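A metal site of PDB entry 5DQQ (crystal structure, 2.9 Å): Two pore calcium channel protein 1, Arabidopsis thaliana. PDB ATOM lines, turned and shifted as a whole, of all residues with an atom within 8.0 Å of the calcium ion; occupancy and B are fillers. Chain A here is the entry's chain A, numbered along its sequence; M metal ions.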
ATOM      1  N   PHE A 321      17.816 -18.531 -31.431  1.00  0.00           N
ATOM      2  CA  PHE A 321      17.289 -17.314 -30.837  1.00  0.00           C
ATOM      3  C   PHE A 321      16.297 -16.630 -31.769  1.00  0.00           C
ATOM      4  O   PHE A 321      15.168 -16.321 -31.373  1.00  0.00           O
ATOM      5  CB  PHE A 321      18.417 -16.351 -30.476  1.00  0.00           C
ATOM      6  CG  PHE A 321      17.924 -14.972 -30.096  1.00  0.00           C
ATOM      7  CD1 PHE A 321      17.674 -14.017 -31.073  1.00  0.00           C
ATOM      8  CD2 PHE A 321      17.686 -14.647 -28.772  1.00  0.00           C
ATOM      9  CE1 PHE A 321      17.211 -12.768 -30.734  1.00  0.00           C
ATOM     10  CE2 PHE A 321      17.223 -13.398 -28.432  1.00  0.00           C
ATOM     11  CZ  PHE A 321      16.988 -12.459 -29.409  1.00  0.00           C
ATOM     12  N   ILE A 324      13.060 -18.002 -31.553  1.00  0.00           N
ATOM     13  CA  ILE A 324      12.311 -17.664 -30.350  1.00  0.00           C
ATOM     14  C   ILE A 324      11.776 -16.241 -30.442  1.00  0.00           C
ATOM     15  O   ILE A 324      10.678 -15.936 -29.946  1.00  0.00           O
ATOM     16  CB  ILE A 324      13.186 -17.856 -29.093  1.00  0.00           C
ATOM     17  CG1 ILE A 324      12.315 -18.315 -27.914  1.00  0.00           C
ATOM     18  CG2 ILE A 324      13.916 -16.571 -28.737  1.00  0.00           C
ATOM     19  CD1 ILE A 324      13.121 -18.770 -26.701  1.00  0.00           C
ATOM     20  N   ASP A 325      12.528 -15.342 -31.071  1.00  0.00           N
ATOM     21  CA  ASP A 325      12.171 -13.929 -31.136  1.00  0.00           C
ATOM     22  C   ASP A 325      11.243 -13.726 -32.334  1.00  0.00           C
ATOM     23  O   ASP A 325      11.673 -13.410 -33.440  1.00  0.00           O
ATOM     24  CB  ASP A 325      13.423 -13.074 -31.245  1.00  0.00           C
ATOM     25  CG  ASP A 325      13.092 -11.600 -31.369  1.00  0.00           C
ATOM     26  OD1 ASP A 325      12.336 -11.095 -30.521  1.00  0.00           O
ATOM     27  OD2 ASP A 325      13.599 -10.958 -32.312  1.00  0.00           O
ATOM     28  N   SER A 326       9.947 -13.889 -32.089  1.00  0.00           N
ATOM     29  CA  SER A 326       8.978 -13.761 -33.171  1.00  0.00           C
ATOM     30  C   SER A 326       8.795 -12.298 -33.584  1.00  0.00           C
ATOM     31  O   SER A 326       8.623 -12.003 -34.765  1.00  0.00           O
ATOM     32  CB  SER A 326       7.645 -14.370 -32.753  1.00  0.00           C
ATOM     33  OG  SER A 326       7.273 -13.940 -31.454  1.00  0.00           O
ATOM     34  N   ASP A 327       8.841 -11.380 -32.618  1.00  0.00           N
ATOM     35  CA  ASP A 327       8.508  -9.989 -32.915  1.00  0.00           C
ATOM     36  C   ASP A 327       9.556  -9.322 -33.800  1.00  0.00           C
ATOM     37  O   ASP A 327       9.249  -8.364 -34.502  1.00  0.00           O
ATOM     38  CB  ASP A 327       8.313  -9.214 -31.611  1.00  0.00           C
ATOM     39  CG  ASP A 327       9.192  -9.725 -30.498  1.00  0.00           C
ATOM     40  OD1 ASP A 327       9.735 -10.848 -30.642  1.00  0.00           O
ATOM     41  OD2 ASP A 327       9.331  -9.022 -29.476  1.00  0.00           O
ATOM     42  N   LYS A 328      10.791  -9.815 -33.776  1.00  0.00           N
ATOM     43  CA  LYS A 328      11.928  -9.327 -34.553  1.00  0.00           C
ATOM     44  C   LYS A 328      12.626  -8.134 -33.909  1.00  0.00           C
ATOM     45  O   LYS A 328      13.641  -7.678 -34.453  1.00  0.00           O
ATOM     46  CB  LYS A 328      11.542  -8.931 -35.983  1.00  0.00           C
ATOM     47  CG  LYS A 328      11.596 -10.043 -37.003  1.00  0.00           C
ATOM     48  CD  LYS A 328      11.500  -9.462 -38.406  1.00  0.00           C
ATOM     49  CE  LYS A 328      11.477 -10.553 -39.469  1.00  0.00           C
ATOM     50  NZ  LYS A 328      11.396  -9.980 -40.834  1.00  0.00           N
ATOM     51  N   ASN A 329      12.141  -7.614 -32.781  1.00  0.00           N
ATOM     52  CA  ASN A 329      12.831  -6.505 -32.137  1.00  0.00           C
ATOM     53  C   ASN A 329      14.293  -6.816 -31.831  1.00  0.00           C
ATOM     54  O   ASN A 329      15.091  -5.884 -31.699  1.00  0.00           O
ATOM     55  CB  ASN A 329      12.113  -6.113 -30.843  1.00  0.00           C
ATOM     56  CG  ASN A 329      11.626  -7.330 -30.062  1.00  0.00           C
ATOM     57  OD1 ASN A 329      11.801  -8.466 -30.493  1.00  0.00           O
ATOM     58  ND2 ASN A 329      11.009  -7.082 -28.915  1.00  0.00           N
ATOM     59  N   GLY A 330      14.663  -8.087 -31.741  1.00  0.00           N
ATOM     60  CA  GLY A 330      16.018  -8.474 -31.406  1.00  0.00           C
ATOM     61  C   GLY A 330      16.242  -8.847 -29.953  1.00  0.00           C
ATOM     62  O   GLY A 330      17.400  -9.031 -29.559  1.00  0.00           O
ATOM     63  N   GLU A 331      15.181  -8.959 -29.164  1.00  0.00           N
ATOM     64  CA  GLU A 331      15.293  -9.308 -27.755  1.00  0.00           C
ATOM     65  C   GLU A 331      14.141 -10.238 -27.394  1.00  0.00           C
ATOM     66  O   GLU A 331      13.130 -10.287 -28.090  1.00  0.00           O
ATOM     67  CB  GLU A 331      15.298  -8.058 -26.872  1.00  0.00           C
ATOM     68  CG  GLU A 331      16.015  -6.870 -27.518  1.00  0.00           C
ATOM     69  CD  GLU A 331      16.598  -5.903 -26.516  1.00  0.00           C
ATOM     70  OE1 GLU A 331      16.406  -6.108 -25.306  1.00  0.00           O
ATOM     71  OE2 GLU A 331      17.274  -4.934 -26.948  1.00  0.00           O
ATOM     72  N   ILE A 332      14.309 -10.980 -26.300  1.00  0.00           N
ATOM     73  CA  ILE A 332      13.366 -12.024 -25.903  1.00  0.00           C
ATOM     74  C   ILE A 332      12.814 -11.677 -24.529  1.00  0.00           C
ATOM     75  O   ILE A 332      13.571 -11.294 -23.620  1.00  0.00           O
ATOM     76  CB  ILE A 332      14.030 -13.400 -25.904  1.00  0.00           C
ATOM     77  N   ASP A 333      11.489 -11.816 -24.371  1.00  0.00           N
ATOM     78  CA  ASP A 333      10.834 -11.444 -23.131  1.00  0.00           C
ATOM     79  C   ASP A 333      11.169 -12.436 -22.020  1.00  0.00           C
ATOM     80  O   ASP A 333      11.516 -13.596 -22.277  1.00  0.00           O
ATOM     81  CB  ASP A 333       9.313 -11.405 -23.323  1.00  0.00           C
ATOM     82  CG  ASP A 333       8.921 -10.867 -24.679  1.00  0.00           C
ATOM     83  OD1 ASP A 333       9.750 -10.209 -25.327  1.00  0.00           O
ATOM     84  OD2 ASP A 333       7.764 -11.117 -25.103  1.00  0.00           O
ATOM     85  N   LYS A 334      11.045 -11.979 -20.772  1.00  0.00           N
ATOM     86  CA  LYS A 334      11.177 -12.896 -19.644  1.00  0.00           C
ATOM     87  C   LYS A 334      10.264 -14.093 -19.826  1.00  0.00           C
ATOM     88  O   LYS A 334      10.709 -15.244 -19.765  1.00  0.00           O
ATOM     89  CB  LYS A 334      10.865 -12.180 -18.329  1.00  0.00           C
ATOM     90  CG  LYS A 334      10.610 -13.138 -17.178  1.00  0.00           C
ATOM     91  CD  LYS A 334       9.960 -12.440 -16.002  1.00  0.00           C
ATOM     92  CE  LYS A 334       8.656 -13.122 -15.609  1.00  0.00           C
ATOM     93  NZ  LYS A 334       7.630 -13.045 -16.693  1.00  0.00           N
ATOM     94  N   GLN A 336       9.070 -15.160 -22.469  1.00  0.00           N
ATOM     95  CA  GLN A 336       9.492 -15.894 -23.654  1.00  0.00           C
ATOM     96  C   GLN A 336      10.704 -16.764 -23.367  1.00  0.00           C
ATOM     97  O   GLN A 336      10.808 -17.885 -23.871  1.00  0.00           O
ATOM     98  CB  GLN A 336       9.783 -14.925 -24.803  1.00  0.00           C
ATOM     99  CG  GLN A 336       9.118 -15.285 -26.116  1.00  0.00           C
ATOM    100  CD  GLN A 336       9.073 -14.123 -27.094  1.00  0.00           C
ATOM    101  OE1 GLN A 336       9.838 -13.166 -26.975  1.00  0.00           O
ATOM    102  NE2 GLN A 336       8.156 -14.192 -28.056  1.00  0.00           N
ATOM    103  N   CYS A 337      11.650 -16.263 -22.562  1.00  0.00           N
ATOM    104  CA  CYS A 337      12.889 -17.000 -22.318  1.00  0.00           C
ATOM    105  C   CYS A 337      12.738 -18.031 -21.193  1.00  0.00           C
ATOM    106  O   CYS A 337      13.485 -19.018 -21.173  1.00  0.00           O
ATOM    107  CB  CYS A 337      14.030 -16.038 -21.990  1.00  0.00           C
ATOM    108  SG  CYS A 337      14.765 -15.208 -23.425  1.00  0.00           S
ATOM    109  N   PHE A 371      13.020  -7.126 -18.602  1.00  0.00           N
ATOM    110  CA  PHE A 371      13.182  -8.538 -18.901  1.00  0.00           C
ATOM    111  C   PHE A 371      13.455  -8.751 -20.395  1.00  0.00           C
ATOM    112  O   PHE A 371      12.769  -9.519 -21.077  1.00  0.00           O
ATOM    113  CB  PHE A 371      11.964  -9.329 -18.439  1.00  0.00           C
ATOM    114  N   LYS A 372      14.463  -8.054 -20.905  1.00  0.00           N
ATOM    115  CA  LYS A 372      14.845  -8.122 -22.305  1.00  0.00           C
ATOM    116  C   LYS A 372      16.300  -8.543 -22.408  1.00  0.00           C
ATOM    117  O   LYS A 372      17.187  -7.856 -21.885  1.00  0.00           O
ATOM    118  CB  LYS A 372      14.603  -6.786 -23.011  1.00  0.00           C
ATOM    119  CG  LYS A 372      13.136  -6.420 -23.048  1.00  0.00           C
ATOM    120  CD  LYS A 372      12.870  -5.076 -23.702  1.00  0.00           C
ATOM    121  CE  LYS A 372      11.419  -4.678 -23.472  1.00  0.00           C
ATOM    122  NZ  LYS A 372      10.989  -3.558 -24.346  1.00  0.00           N
ATOM    123  N   ILE A 373      16.536  -9.675 -23.070  1.00  0.00           N
ATOM    124  CA  ILE A 373      17.870 -10.204 -23.304  1.00  0.00           C
ATOM    125  C   ILE A 373      18.103 -10.228 -24.807  1.00  0.00           C
ATOM    126  O   ILE A 373      17.241 -10.681 -25.568  1.00  0.00           O
ATOM    127  CB  ILE A 373      18.046 -11.603 -22.691  1.00  0.00           C
ATOM    128  CG1 ILE A 373      19.477 -11.799 -22.189  1.00  0.00           C
ATOM    129  CG2 ILE A 373      17.673 -12.682 -23.706  1.00  0.00           C
ATOM    130  CD1 ILE A 373      19.552 -12.506 -20.853  1.00  0.00           C
HETATM  131 CA    CA M   1      10.861 -10.645 -28.385  1.00  0.00          CA
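The backbone NH of Ile 332 sits at hydrogen-bond distance from the backbone carbonyl oxygen of Ile 373 (3.0 Å). The side-chain amide oxygen (OD1) of Asn 329 sits close to the backbone carbonyl oxygen (O) of Glu 331. The side-chain carboxylate of Asp 325 lies within hydrogen-bond range of the backbone NH of Gly 330, at 3.1 Å. OE1 of Gln 336 is in hydrogen-bond range of N of Asp 333 (3.4 Å). The side-chain carboxylate (OD1) of Asp 325 lies close to the side-chain amide oxygen (OD1) of Asn 329. OD2 of Asp 327 lies close to ND2 of Asn 329 (2.6 Å). The side-chain carboxylate of Asp 325 lies close to the backbone NH of Lys 328 (3.4 Å).
Asn 329 touches the calcium ion (OD1 to CA, 3.2 Å). Ile 332 touches the calcium ion (CA to CA, 3.8 Å). Asp 333 touches the calcium ion (OD1 to CA, 3.3 Å). Within 4 Å of the calcium ion: Asp 325, Asp 327, Asn 329, Glu 331, Ile 332, Asp 333 and Gln 336. The nearest printed residue that does not touch the calcium ion is Ser 326 (5.0 Å).
The calcium ion is bound by O of Glu 331 (2.3 Å), OD2 of Asp 327 (2.5 Å), OD1 of Asp 327 (2.5 Å) and OD1 of Asp 325 (2.6 Å). The calcium ion has four donor atoms within binding distance. Slightly farther from the calcium ion lies OE1 of Gln 336 (3.1 Å).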
